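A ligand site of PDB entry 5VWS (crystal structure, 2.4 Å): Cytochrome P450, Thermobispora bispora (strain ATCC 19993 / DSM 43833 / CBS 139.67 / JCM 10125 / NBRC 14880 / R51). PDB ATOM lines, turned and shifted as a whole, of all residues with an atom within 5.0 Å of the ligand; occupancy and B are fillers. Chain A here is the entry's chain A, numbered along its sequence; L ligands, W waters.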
ATOM      1  N   LEU A  53      -9.376  -8.094  -1.486  1.00  0.00           N
ATOM      2  CA  LEU A  53      -8.050  -8.376  -2.021  1.00  0.00           C
ATOM      3  C   LEU A  53      -7.339  -7.101  -2.462  1.00  0.00           C
ATOM      4  O   LEU A  53      -6.112  -6.985  -2.304  1.00  0.00           O
ATOM      5  CB  LEU A  53      -8.154  -9.369  -3.166  1.00  0.00           C
ATOM      6  CG  LEU A  53      -8.454 -10.791  -2.702  1.00  0.00           C
ATOM      7  CD1 LEU A  53      -8.475 -11.743  -3.871  1.00  0.00           C
ATOM      8  CD2 LEU A  53      -7.444 -11.231  -1.688  1.00  0.00           C
ATOM      9  N   ILE A  78       7.693  -9.907  -0.079  1.00  0.00           N
ATOM     10  CA  ILE A  78       6.578  -9.159  -0.647  1.00  0.00           C
ATOM     11  C   ILE A  78       5.220  -9.741  -0.272  1.00  0.00           C
ATOM     12  O   ILE A  78       4.243  -9.007  -0.183  1.00  0.00           O
ATOM     13  CB  ILE A  78       6.754  -9.027  -2.174  1.00  0.00           C
ATOM     14  CG1 ILE A  78       6.639 -10.376  -2.884  1.00  0.00           C
ATOM     15  CG2 ILE A  78       8.117  -8.445  -2.485  1.00  0.00           C
ATOM     16  CD1 ILE A  78       7.012 -10.284  -4.352  1.00  0.00           C
ATOM     17  N   THR A  79       5.134 -11.046  -0.024  1.00  0.00           N
ATOM     18  CA  THR A  79       3.820 -11.581   0.352  1.00  0.00           C
ATOM     19  C   THR A  79       3.376 -11.158   1.740  1.00  0.00           C
ATOM     20  O   THR A  79       2.226 -11.437   2.116  1.00  0.00           O
ATOM     21  CB  THR A  79       3.817 -13.114   0.297  1.00  0.00           C
ATOM     22  OG1 THR A  79       4.701 -13.618   1.301  1.00  0.00           O
ATOM     23  CG2 THR A  79       4.208 -13.635  -1.091  1.00  0.00           C
ATOM     24  N   HIS A  86       6.057  -2.532   0.245  1.00  0.00           N
ATOM     25  CA  HIS A  86       5.725  -3.561  -0.734  1.00  0.00           C
ATOM     26  C   HIS A  86       5.918  -3.071  -2.165  1.00  0.00           C
ATOM     27  O   HIS A  86       6.376  -3.835  -3.025  1.00  0.00           O
ATOM     28  CB  HIS A  86       4.294  -4.021  -0.528  1.00  0.00           C
ATOM     29  CG  HIS A  86       3.857  -5.080  -1.485  1.00  0.00           C
ATOM     30  ND1 HIS A  86       3.577  -4.807  -2.809  1.00  0.00           N
ATOM     31  CD2 HIS A  86       3.668  -6.406  -1.324  1.00  0.00           C
ATOM     32  CE1 HIS A  86       3.226  -5.917  -3.418  1.00  0.00           C
ATOM     33  NE2 HIS A  86       3.264  -6.906  -2.540  1.00  0.00           N
ATOM     34  N   ARG A  90       8.766  -4.811  -4.722  1.00  0.00           N
ATOM     35  CA  ARG A  90       8.306  -5.584  -5.866  1.00  0.00           C
ATOM     36  C   ARG A  90       8.695  -4.948  -7.192  1.00  0.00           C
ATOM     37  O   ARG A  90       8.705  -5.632  -8.217  1.00  0.00           O
ATOM     38  CB  ARG A  90       6.795  -5.792  -5.806  1.00  0.00           C
ATOM     39  CG  ARG A  90       6.183  -6.320  -7.098  1.00  0.00           C
ATOM     40  CD  ARG A  90       4.747  -6.809  -6.838  1.00  0.00           C
ATOM     41  NE  ARG A  90       4.031  -7.224  -8.040  1.00  0.00           N
ATOM     42  CZ  ARG A  90       3.121  -8.184  -8.039  1.00  0.00           C
ATOM     43  NH1 ARG A  90       2.839  -8.823  -6.909  1.00  0.00           N
ATOM     44  NH2 ARG A  90       2.486  -8.525  -9.163  1.00  0.00           N
ATOM     45  N   PHE A  97      12.248  -9.536 -13.366  1.00  0.00           N
ATOM     46  CA  PHE A  97      11.215 -10.480 -13.792  1.00  0.00           C
ATOM     47  C   PHE A  97      10.373  -9.885 -14.926  1.00  0.00           C
ATOM     48  O   PHE A  97       9.160  -9.691 -14.815  1.00  0.00           O
ATOM     49  CB  PHE A  97      10.346 -10.857 -12.596  1.00  0.00           C
ATOM     50  CG  PHE A  97       9.706 -12.204 -12.727  1.00  0.00           C
ATOM     51  CD1 PHE A  97      10.480 -13.344 -12.937  1.00  0.00           C
ATOM     52  CD2 PHE A  97       8.328 -12.356 -12.616  1.00  0.00           C
ATOM     53  CE1 PHE A  97       9.903 -14.586 -13.047  1.00  0.00           C
ATOM     54  CE2 PHE A  97       7.743 -13.607 -12.733  1.00  0.00           C
ATOM     55  CZ  PHE A  97       8.532 -14.718 -12.940  1.00  0.00           C
ATOM     56  N   ILE A 140      11.410 -23.211 -13.010  1.00  0.00           N
ATOM     57  CA  ILE A 140      12.012 -22.257 -12.086  1.00  0.00           C
ATOM     58  C   ILE A 140      13.525 -22.428 -12.060  1.00  0.00           C
ATOM     59  O   ILE A 140      14.286 -21.460 -12.127  1.00  0.00           O
ATOM     60  CB  ILE A 140      11.400 -22.447 -10.686  1.00  0.00           C
ATOM     61  CG1 ILE A 140       9.898 -22.311 -10.808  1.00  0.00           C
ATOM     62  CG2 ILE A 140      11.918 -21.398  -9.760  1.00  0.00           C
ATOM     63  CD1 ILE A 140       9.491 -20.965 -11.345  1.00  0.00           C
ATOM     64  N   LEU A 229      11.204 -17.924  -2.918  1.00  0.00           N
ATOM     65  CA  LEU A 229       9.782 -17.615  -3.010  1.00  0.00           C
ATOM     66  C   LEU A 229       9.187 -18.068  -4.329  1.00  0.00           C
ATOM     67  O   LEU A 229       8.071 -18.607  -4.355  1.00  0.00           O
ATOM     68  CB  LEU A 229       9.531 -16.124  -2.806  1.00  0.00           C
ATOM     69  CG  LEU A 229       8.078 -15.689  -3.039  1.00  0.00           C
ATOM     70  CD1 LEU A 229       7.123 -16.586  -2.289  1.00  0.00           C
ATOM     71  CD2 LEU A 229       7.838 -14.237  -2.661  1.00  0.00           C
ATOM     72  N   LEU A 230       9.889 -17.858  -5.443  1.00  0.00           N
ATOM     73  CA  LEU A 230       9.350 -18.247  -6.739  1.00  0.00           C
ATOM     74  C   LEU A 230       9.179 -19.759  -6.810  1.00  0.00           C
ATOM     75  O   LEU A 230       8.086 -20.266  -7.098  1.00  0.00           O
ATOM     76  CB  LEU A 230      10.274 -17.745  -7.844  1.00  0.00           C
ATOM     77  CG  LEU A 230      10.623 -16.280  -7.667  1.00  0.00           C
ATOM     78  CD1 LEU A 230      11.900 -15.927  -8.411  1.00  0.00           C
ATOM     79  CD2 LEU A 230       9.475 -15.477  -8.191  1.00  0.00           C
ATOM     80  N   ALA A 233       6.217 -20.729  -4.893  1.00  0.00           N
ATOM     81  CA  ALA A 233       4.939 -20.109  -5.249  1.00  0.00           C
ATOM     82  C   ALA A 233       4.437 -20.550  -6.612  1.00  0.00           C
ATOM     83  O   ALA A 233       3.228 -20.704  -6.788  1.00  0.00           O
ATOM     84  CB  ALA A 233       5.051 -18.576  -5.229  1.00  0.00           C
ATOM     85  N   GLY A 234       5.335 -20.753  -7.558  1.00  0.00           N
ATOM     86  CA  GLY A 234       4.988 -21.143  -8.904  1.00  0.00           C
ATOM     87  C   GLY A 234       5.001 -22.615  -9.148  1.00  0.00           C
ATOM     88  O   GLY A 234       4.664 -23.056 -10.249  1.00  0.00           O
ATOM     89  N   THR A 237       1.058 -24.645  -7.526  1.00  0.00           N
ATOM     90  CA  THR A 237      -0.043 -23.980  -8.206  1.00  0.00           C
ATOM     91  C   THR A 237      -0.097 -24.364  -9.679  1.00  0.00           C
ATOM     92  O   THR A 237      -1.159 -24.701 -10.205  1.00  0.00           O
ATOM     93  CB  THR A 237       0.028 -22.466  -8.058  1.00  0.00           C
ATOM     94  OG1 THR A 237       1.322 -21.988  -8.454  1.00  0.00           O
ATOM     95  CG2 THR A 237      -0.273 -22.057  -6.633  1.00  0.00           C
ATOM     96  N   THR A 238       1.060 -24.347 -10.378  1.00  0.00           N
ATOM     97  CA  THR A 238       1.077 -24.766 -11.782  1.00  0.00           C
ATOM     98  C   THR A 238       0.782 -26.268 -11.938  1.00  0.00           C
ATOM     99  O   THR A 238       0.111 -26.675 -12.899  1.00  0.00           O
ATOM    100  CB  THR A 238       2.416 -24.433 -12.423  1.00  0.00           C
ATOM    101  OG1 THR A 238       2.732 -23.051 -12.219  1.00  0.00           O
ATOM    102  CG2 THR A 238       2.374 -24.753 -13.915  1.00  0.00           C
ATOM    103  N   LEU A 241      -2.836 -26.730 -11.919  1.00  0.00           N
ATOM    104  CA  LEU A 241      -3.378 -26.137 -13.139  1.00  0.00           C
ATOM    105  C   LEU A 241      -3.318 -27.117 -14.291  1.00  0.00           C
ATOM    106  O   LEU A 241      -4.265 -27.204 -15.072  1.00  0.00           O
ATOM    107  CB  LEU A 241      -2.632 -24.875 -13.509  1.00  0.00           C
ATOM    108  CG  LEU A 241      -3.097 -24.260 -14.819  1.00  0.00           C
ATOM    109  CD1 LEU A 241      -4.476 -23.677 -14.674  1.00  0.00           C
ATOM    110  CD2 LEU A 241      -2.135 -23.192 -15.248  1.00  0.00           C
ATOM    111  N   LEU A 274      -8.796 -22.455 -14.693  1.00  0.00           N
ATOM    112  CA  LEU A 274      -8.463 -21.510 -13.627  1.00  0.00           C
ATOM    113  C   LEU A 274      -9.692 -21.027 -12.864  1.00  0.00           C
ATOM    114  O   LEU A 274      -9.666 -20.949 -11.622  1.00  0.00           O
ATOM    115  CB  LEU A 274      -7.696 -20.324 -14.226  1.00  0.00           C
ATOM    116  CG  LEU A 274      -6.223 -20.647 -14.430  1.00  0.00           C
ATOM    117  CD1 LEU A 274      -5.606 -19.683 -15.419  1.00  0.00           C
ATOM    118  CD2 LEU A 274      -5.469 -20.609 -13.104  1.00  0.00           C
ATOM    119  N   PRO A 279      -6.416 -23.070  -8.666  1.00  0.00           N
ATOM    120  CA  PRO A 279      -5.393 -23.705  -7.828  1.00  0.00           C
ATOM    121  C   PRO A 279      -5.352 -23.193  -6.396  1.00  0.00           C
ATOM    122  O   PRO A 279      -5.187 -23.991  -5.479  1.00  0.00           O
ATOM    123  CB  PRO A 279      -4.089 -23.382  -8.581  1.00  0.00           C
ATOM    124  CG  PRO A 279      -4.506 -23.203  -9.976  1.00  0.00           C
ATOM    125  CD  PRO A 279      -5.843 -22.512  -9.886  1.00  0.00           C
ATOM    126  N   PHE A 280      -5.481 -21.892  -6.183  1.00  0.00           N
ATOM    127  CA  PHE A 280      -5.397 -21.317  -4.836  1.00  0.00           C
ATOM    128  C   PHE A 280      -6.795 -21.124  -4.289  1.00  0.00           C
ATOM    129  O   PHE A 280      -7.593 -20.372  -4.857  1.00  0.00           O
ATOM    130  CB  PHE A 280      -4.641 -20.003  -4.849  1.00  0.00           C
ATOM    131  CG  PHE A 280      -3.585 -19.914  -3.796  1.00  0.00           C
ATOM    132  CD1 PHE A 280      -2.456 -20.709  -3.872  1.00  0.00           C
ATOM    133  CD2 PHE A 280      -3.738 -19.072  -2.702  1.00  0.00           C
ATOM    134  CE1 PHE A 280      -1.478 -20.646  -2.889  1.00  0.00           C
ATOM    135  CE2 PHE A 280      -2.780 -19.000  -1.706  1.00  0.00           C
ATOM    136  CZ  PHE A 280      -1.639 -19.792  -1.799  1.00  0.00           C
ATOM    137  N   ALA A 283      -7.341 -16.710   0.366  1.00  0.00           N
ATOM    138  CA  ALA A 283      -6.295 -15.750   0.632  1.00  0.00           C
ATOM    139  C   ALA A 283      -6.647 -15.086   1.943  1.00  0.00           C
ATOM    140  O   ALA A 283      -7.808 -14.762   2.170  1.00  0.00           O
ATOM    141  CB  ALA A 283      -6.175 -14.709  -0.485  1.00  0.00           C
ATOM    142  N   ARG A 285      -6.044 -12.160   4.938  1.00  0.00           N
ATOM    143  CA  ARG A 285      -5.586 -10.843   5.368  1.00  0.00           C
ATOM    144  C   ARG A 285      -5.972 -10.637   6.817  1.00  0.00           C
ATOM    145  O   ARG A 285      -6.877 -11.289   7.352  1.00  0.00           O
ATOM    146  CB  ARG A 285      -6.202  -9.747   4.505  1.00  0.00           C
ATOM    147  CG  ARG A 285      -5.985  -9.942   3.038  1.00  0.00           C
ATOM    148  CD  ARG A 285      -4.606  -9.488   2.636  1.00  0.00           C
ATOM    149  NE  ARG A 285      -4.471  -9.399   1.197  1.00  0.00           N
ATOM    150  CZ  ARG A 285      -4.099 -10.404   0.406  1.00  0.00           C
ATOM    151  NH1 ARG A 285      -3.806 -11.591   0.933  1.00  0.00           N
ATOM    152  NH2 ARG A 285      -4.019 -10.221  -0.912  1.00  0.00           N
ATOM    153  N   ILE A 308     -11.182 -17.245  -2.673  1.00  0.00           N
ATOM    154  CA  ILE A 308     -10.975 -17.099  -4.115  1.00  0.00           C
ATOM    155  C   ILE A 308     -11.798 -18.115  -4.906  1.00  0.00           C
ATOM    156  O   ILE A 308     -12.206 -17.837  -6.037  1.00  0.00           O
ATOM    157  CB  ILE A 308      -9.470 -17.221  -4.444  1.00  0.00           C
ATOM    158  CG1 ILE A 308      -8.742 -15.950  -4.065  1.00  0.00           C
ATOM    159  CG2 ILE A 308      -9.276 -17.528  -5.904  1.00  0.00           C
ATOM    160  CD1 ILE A 308      -7.245 -16.025  -4.245  1.00  0.00           C
ATOM    161  N   ILE A 334     -10.702 -14.239 -10.343  1.00  0.00           N
ATOM    162  CA  ILE A 334      -9.605 -13.806  -9.485  1.00  0.00           C
ATOM    163  C   ILE A 334      -8.759 -14.987  -9.037  1.00  0.00           C
ATOM    164  O   ILE A 334      -8.179 -14.973  -7.945  1.00  0.00           O
ATOM    165  CB  ILE A 334     -10.102 -12.997  -8.268  1.00  0.00           C
ATOM    166  CG1 ILE A 334     -11.264 -13.705  -7.564  1.00  0.00           C
ATOM    167  CG2 ILE A 334     -10.524 -11.606  -8.699  1.00  0.00           C
ATOM    168  CD1 ILE A 334     -11.526 -13.155  -6.143  1.00  0.00           C
ATOM    169  N   ALA A 335      -8.650 -15.999  -9.890  1.00  0.00           N
ATOM    170  CA  ALA A 335      -7.729 -17.103  -9.625  1.00  0.00           C
ATOM    171  C   ALA A 335      -6.337 -16.606  -9.241  1.00  0.00           C
ATOM    172  O   ALA A 335      -5.754 -17.089  -8.273  1.00  0.00           O
ATOM    173  CB  ALA A 335      -7.645 -18.011 -10.849  1.00  0.00           C
ATOM    174  N   PHE A 336      -5.781 -15.640  -9.978  1.00  0.00           N
ATOM    175  CA  PHE A 336      -4.481 -15.083  -9.625  1.00  0.00           C
ATOM    176  C   PHE A 336      -4.569 -13.912  -8.639  1.00  0.00           C
ATOM    177  O   PHE A 336      -3.537 -13.292  -8.342  1.00  0.00           O
ATOM    178  CB  PHE A 336      -3.726 -14.602 -10.862  1.00  0.00           C
ATOM    179  CG  PHE A 336      -3.463 -15.664 -11.883  1.00  0.00           C
ATOM    180  CD1 PHE A 336      -2.383 -16.520 -11.758  1.00  0.00           C
ATOM    181  CD2 PHE A 336      -4.272 -15.775 -13.001  1.00  0.00           C
ATOM    182  CE1 PHE A 336      -2.134 -17.471 -12.713  1.00  0.00           C
ATOM    183  CE2 PHE A 336      -4.024 -16.745 -13.960  1.00  0.00           C
ATOM    184  CZ  PHE A 336      -2.949 -17.582 -13.822  1.00  0.00           C
ATOM    185  N   GLY A 337      -5.763 -13.601  -8.131  1.00  0.00           N
ATOM    186  CA  GLY A 337      -5.923 -12.544  -7.173  1.00  0.00           C
ATOM    187  C   GLY A 337      -6.363 -11.211  -7.735  1.00  0.00           C
ATOM    188  O   GLY A 337      -7.032 -11.118  -8.777  1.00  0.00           O
ATOM    189  N   VAL A 340      -2.387  -5.066  -5.342  1.00  0.00           N
ATOM    190  CA  VAL A 340      -0.932  -4.928  -5.389  1.00  0.00           C
ATOM    191  C   VAL A 340      -0.219  -6.255  -5.249  1.00  0.00           C
ATOM    192  O   VAL A 340       0.966  -6.348  -5.600  1.00  0.00           O
ATOM    193  CB  VAL A 340      -0.447  -3.979  -4.278  1.00  0.00           C
ATOM    194  CG1 VAL A 340      -0.799  -2.553  -4.570  1.00  0.00           C
ATOM    195  CG2 VAL A 340      -1.055  -4.390  -2.953  1.00  0.00           C
ATOM    196  N   HIS A 341      -0.881  -7.268  -4.690  1.00  0.00           N
ATOM    197  CA  HIS A 341      -0.306  -8.589  -4.486  1.00  0.00           C
ATOM    198  C   HIS A 341      -0.621  -9.566  -5.605  1.00  0.00           C
ATOM    199  O   HIS A 341      -0.087 -10.679  -5.598  1.00  0.00           O
ATOM    200  CB  HIS A 341      -0.789  -9.209  -3.163  1.00  0.00           C
ATOM    201  CG  HIS A 341      -0.193  -8.579  -1.930  1.00  0.00           C
ATOM    202  ND1 HIS A 341       1.110  -8.776  -1.563  1.00  0.00           N
ATOM    203  CD2 HIS A 341      -0.744  -7.782  -0.997  1.00  0.00           C
ATOM    204  CE1 HIS A 341       1.348  -8.110  -0.441  1.00  0.00           C
ATOM    205  NE2 HIS A 341       0.240  -7.496  -0.078  1.00  0.00           N
ATOM    206  N   PHE A 342      -1.470  -9.173  -6.562  1.00  0.00           N
ATOM    207  CA  PHE A 342      -1.739  -9.976  -7.761  1.00  0.00           C
ATOM    208  C   PHE A 342      -0.516 -10.780  -8.178  1.00  0.00           C
ATOM    209  O   PHE A 342       0.612 -10.281  -8.160  1.00  0.00           O
ATOM    210  CB  PHE A 342      -2.183  -9.085  -8.910  1.00  0.00           C
ATOM    211  CG  PHE A 342      -2.586  -9.847 -10.135  1.00  0.00           C
ATOM    212  CD1 PHE A 342      -3.868 -10.286 -10.289  1.00  0.00           C
ATOM    213  CD2 PHE A 342      -1.663 -10.114 -11.133  1.00  0.00           C
ATOM    214  CE1 PHE A 342      -4.230 -10.985 -11.416  1.00  0.00           C
ATOM    215  CE2 PHE A 342      -2.025 -10.813 -12.260  1.00  0.00           C
ATOM    216  CZ  PHE A 342      -3.304 -11.244 -12.398  1.00  0.00           C
ATOM    217  N   CYS A 343      -0.749 -12.034  -8.564  1.00  0.00           N
ATOM    218  CA  CYS A 343       0.319 -13.015  -8.721  1.00  0.00           C
ATOM    219  C   CYS A 343       1.417 -12.504  -9.630  1.00  0.00           C
ATOM    220  O   CYS A 343       1.183 -12.179 -10.792  1.00  0.00           O
ATOM    221  CB  CYS A 343      -0.264 -14.304  -9.282  1.00  0.00           C
ATOM    222  SG  CYS A 343       1.002 -15.477  -9.815  1.00  0.00           S
ATOM    223  N   LEU A 344       2.639 -12.459  -9.103  1.00  0.00           N
ATOM    224  CA  LEU A 344       3.750 -11.998  -9.899  1.00  0.00           C
ATOM    225  C   LEU A 344       4.136 -12.971 -11.008  1.00  0.00           C
ATOM    226  O   LEU A 344       4.920 -12.611 -11.885  1.00  0.00           O
ATOM    227  CB  LEU A 344       4.941 -11.741  -8.987  1.00  0.00           C
ATOM    228  CG  LEU A 344       6.132 -11.177  -9.751  1.00  0.00           C
ATOM    229  CD1 LEU A 344       5.809  -9.742 -10.047  1.00  0.00           C
ATOM    230  CD2 LEU A 344       7.436 -11.341  -8.962  1.00  0.00           C
ATOM    231  N   GLY A 345       3.603 -14.194 -10.998  1.00  0.00           N
ATOM    232  CA  GLY A 345       3.978 -15.179 -11.969  1.00  0.00           C
ATOM    233  C   GLY A 345       2.891 -15.596 -12.927  1.00  0.00           C
ATOM    234  O   GLY A 345       3.104 -16.471 -13.776  1.00  0.00           O
ATOM    235  N   ALA A 346       1.699 -14.986 -12.820  1.00  0.00           N
ATOM    236  CA  ALA A 346       0.584 -15.432 -13.655  1.00  0.00           C
ATOM    237  C   ALA A 346       1.022 -15.601 -15.100  1.00  0.00           C
ATOM    238  O   ALA A 346       0.742 -16.621 -15.722  1.00  0.00           O
ATOM    239  CB  ALA A 346      -0.588 -14.446 -13.559  1.00  0.00           C
ATOM    240  N   LEU A 348       3.935 -16.256 -16.379  1.00  0.00           N
ATOM    241  CA  LEU A 348       4.709 -17.487 -16.467  1.00  0.00           C
ATOM    242  C   LEU A 348       3.822 -18.713 -16.275  1.00  0.00           C
ATOM    243  O   LEU A 348       3.953 -19.704 -17.012  1.00  0.00           O
ATOM    244  CB  LEU A 348       5.825 -17.480 -15.431  1.00  0.00           C
ATOM    245  CG  LEU A 348       6.516 -18.837 -15.408  1.00  0.00           C
ATOM    246  CD1 LEU A 348       7.171 -19.032 -16.767  1.00  0.00           C
ATOM    247  CD2 LEU A 348       7.499 -18.902 -14.266  1.00  0.00           C
ATOM    248  N   GLY A 349       2.937 -18.680 -15.282  1.00  0.00           N
ATOM    249  CA  GLY A 349       2.079 -19.826 -15.024  1.00  0.00           C
ATOM    250  C   GLY A 349       1.235 -20.205 -16.225  1.00  0.00           C
ATOM    251  O   GLY A 349       1.185 -21.362 -16.644  1.00  0.00           O
ATOM    252  N   GLU A 352       3.486 -21.848 -18.940  1.00  0.00           N
ATOM    253  CA  GLU A 352       3.752 -23.242 -18.568  1.00  0.00           C
ATOM    254  C   GLU A 352       2.565 -24.133 -18.898  1.00  0.00           C
ATOM    255  O   GLU A 352       2.709 -25.131 -19.602  1.00  0.00           O
ATOM    256  CB  GLU A 352       4.086 -23.341 -17.086  1.00  0.00           C
ATOM    257  CG  GLU A 352       5.561 -23.071 -16.771  1.00  0.00           C
ATOM    258  CD  GLU A 352       5.898 -23.386 -15.327  1.00  0.00           C
ATOM    259  OE1 GLU A 352       5.412 -24.440 -14.823  1.00  0.00           O
ATOM    260  OE2 GLU A 352       6.650 -22.594 -14.701  1.00  0.00           O
HETATM  261  C1  LIG L   1       0.743 -14.528  -5.583  1.00  0.00           C
HETATM  262  C2  LIG L   1      -2.070 -17.828  -7.739  1.00  0.00           C
HETATM  263  C3  LIG L   1       1.768 -19.251 -10.300  1.00  0.00           C
HETATM  264  C4  LIG L   1       4.622 -16.252  -7.934  1.00  0.00           C
HETATM  265  C5  LIG L   1      -0.347 -15.266  -5.948  1.00  0.00           C
HETATM  266  C6  LIG L   1      -1.706 -15.048  -5.506  1.00  0.00           C
HETATM  267  C7  LIG L   1      -2.466 -15.953  -6.128  1.00  0.00           C
HETATM  268  C8  LIG L   1      -1.638 -16.790  -6.960  1.00  0.00           C
HETATM  269  C9  LIG L   1      -3.981 -16.115  -5.979  1.00  0.00           C
HETATM  270  C10 LIG L   1      -2.188 -13.925  -4.543  1.00  0.00           C
HETATM  271  C11 LIG L   1      -1.900 -14.163  -3.062  1.00  0.00           C
HETATM  272  C12 LIG L   1      -2.486 -13.046  -2.270  1.00  0.00           C
HETATM  273  O1  LIG L   1      -2.953 -12.041  -2.870  1.00  0.00           O
HETATM  274  O2  LIG L   1      -2.499 -13.139  -1.029  1.00  0.00           O
HETATM  275  C13 LIG L   1      -1.289 -18.457  -8.649  1.00  0.00           C
HETATM  276  C14 LIG L   1      -1.740 -19.422  -9.616  1.00  0.00           C
HETATM  277  C15 LIG L   1      -0.642 -19.797 -10.322  1.00  0.00           C
HETATM  278  C16 LIG L   1       0.497 -19.096  -9.805  1.00  0.00           C
HETATM  279  C17 LIG L   1      -3.224 -19.826  -9.734  1.00  0.00           C
HETATM  280  C18 LIG L   1      -0.441 -20.782 -11.486  1.00  0.00           C
HETATM  281  C19 LIG L   1      -1.360 -21.617 -11.929  1.00  0.00           C
HETATM  282  C20 LIG L   1       2.867 -18.556  -9.922  1.00  0.00           C
HETATM  283  C21 LIG L   1       4.174 -18.640 -10.543  1.00  0.00           C
HETATM  284  C22 LIG L   1       4.967 -17.793  -9.892  1.00  0.00           C
HETATM  285  C23 LIG L   1       4.197 -17.177  -8.841  1.00  0.00           C
HETATM  286  C24 LIG L   1       4.458 -19.537 -11.773  1.00  0.00           C
HETATM  287  C25 LIG L   1       6.434 -17.488 -10.154  1.00  0.00           C
HETATM  288  C26 LIG L   1       7.233 -18.281 -10.877  1.00  0.00           C
HETATM  289  C27 LIG L   1       3.808 -15.517  -7.094  1.00  0.00           C
HETATM  290  C28 LIG L   1       4.259 -14.473  -6.178  1.00  0.00           C
HETATM  291  C29 LIG L   1       3.178 -13.996  -5.545  1.00  0.00           C
HETATM  292  C30 LIG L   1       2.025 -14.724  -6.014  1.00  0.00           C
HETATM  293  C31 LIG L   1       5.724 -14.027  -6.006  1.00  0.00           C
HETATM  294  C32 LIG L   1       3.127 -12.893  -4.469  1.00  0.00           C
HETATM  295  C33 LIG L   1       3.021 -11.491  -5.059  1.00  0.00           C
HETATM  296  C34 LIG L   1       2.911 -10.461  -3.947  1.00  0.00           C
HETATM  297  O3  LIG L   1       2.767 -10.852  -2.763  1.00  0.00           O
HETATM  298  O4  LIG L   1       2.965  -9.249  -4.242  1.00  0.00           O
HETATM  299  N1  LIG L   1      -0.347 -16.338  -6.835  1.00  0.00           N
HETATM  300  N2  LIG L   1       0.072 -18.270  -8.780  1.00  0.00           N
HETATM  301  N3  LIG L   1       2.921 -17.654  -8.885  1.00  0.00           N
HETATM  302  N4  LIG L   1       2.436 -15.655  -6.952  1.00  0.00           N
HETATM  303 FE1  LIG L   1       1.208 -16.874  -7.930  1.00  0.00          FE
HETATM  304  O   HOH W   1       1.472 -18.466  -4.754  1.00  0.00           O
HETATM  305  O   HOH W   2      -4.022 -10.438  -4.582  1.00  0.00           O
HETATM  306  O   HOH W   3       0.096 -12.208  -1.368  1.00  0.00           O
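NH1 of Arg 90 sits at hydrogen-bond distance from O of Val 340 (3.4 Å).
OG1 of Thr 238 lies within hydrogen-bond range of O of Gly 234 (2.8 Å).
The guanidinium group (NH2) of Arg 90 sits at hydrogen-bond distance from the backbone carbonyl oxygen (O) of Phe 342 (2.8 Å).
A ring nitrogen (NE2) of His 86 sits close to the backbone carbonyl oxygen of Ile 78 (3.3 Å).
A ring nitrogen (NE2) of His 86 is in hydrogen-bond range of a ring nitrogen (ND1) of His 341.
The side-chain sulfur (SG) of Cys 343 sits close to the backbone NH (N) of Ala 346 (3.1 Å).
The backbone carbonyl oxygen (O) of Ala 233 is in hydrogen-bond range of the side-chain hydroxyl (OG1) of Thr 237 (2.8 Å).
The backbone NH (N) of Cys 343 sits at hydrogen-bond distance from the backbone carbonyl oxygen (O) of Phe 336, 3.1 Å away.
O of Ile 78 lies close to O3 of the ligand, 3.5 Å away.
Thr 79 touches the ligand (CA to O3, 3.4 Å).
Ile 140 touches the ligand.
CD2 of Leu 229 touches C31 of the ligand (3.96 Å).
Ala 233 touches the ligand (CB to C4, 3.6 Å).
Gly 234 touches the ligand.
Thr 237 touches the ligand (OG1 to C16, 3.3 Å).
Thr 238 touches the ligand (OG1 to C24, 3.9 Å).
Leu 241 touches the ligand.
CG of Pro 279 touches C17 of the ligand, 3.6 Å away.
Ile 308 touches the ligand.
Ala 335 touches the ligand (O to C9, 3.1 Å).
C of Phe 336 touches C9 of the ligand, at 3.5 Å.
N of Gly 337 touches C9 of the ligand, at 3.8 Å.
Val 340 touches the ligand.
CB of Leu 344 touches C31 of the ligand (3.8 Å).
CA of Gly 345 touches C22 of the ligand, 3.5 Å away.
CD2 of Leu 348 touches C26 of the ligand, at 3.5 Å.
Gly 349 touches the ligand (N to C24, 3.9 Å).
Hydrophobic or aromatic side chains within 4 Å of the ligand: Ile 78, His 86, Ile 140, Leu 229, Ala 233, Leu 241, Pro 279, Ile 308, Phe 336, His 341, Leu 344 and Leu 348.
24 residues have an atom within 4 Å of the ligand: Ile 78, Thr 79, His 86, Arg 90, Ile 140, Leu 229, Ala 233, Gly 234, Thr 237, Thr 238, Leu 241, Pro 279, Arg 285, Ile 308, Ala 335, Phe 336, Gly 337, Val 340, His 341, Cys 343, Leu 344, Gly 345, Leu 348 and Gly 349.
Along chain A the residues within 4 Å of the ligand span positions 78 to 349.
The nearest printed residue that does not touch the ligand is Ala 283 (4.03 Å).
Water W2 bridges O1 of the ligand (2.6 Å) and N of Phe 342 (3.5 Å).
The guanidinium group (NH1) of Arg 90 lies within salt-bridge range of an oxygen (O4) of the ligand (2.7 Å).
NE2 of His 86 sits at hydrogen-bond distance from O4 of the ligand (2.9 Å).
ND1 of His 341 is in hydrogen-bond range of O3 of the ligand (2.9 Å).
The side-chain sulfur (SG) of Cys 343 binds an iron atom (FE1) of the ligand, at 2.4 Å.
O2 of the ligand is in salt-bridge range of NH1 of Arg 285.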
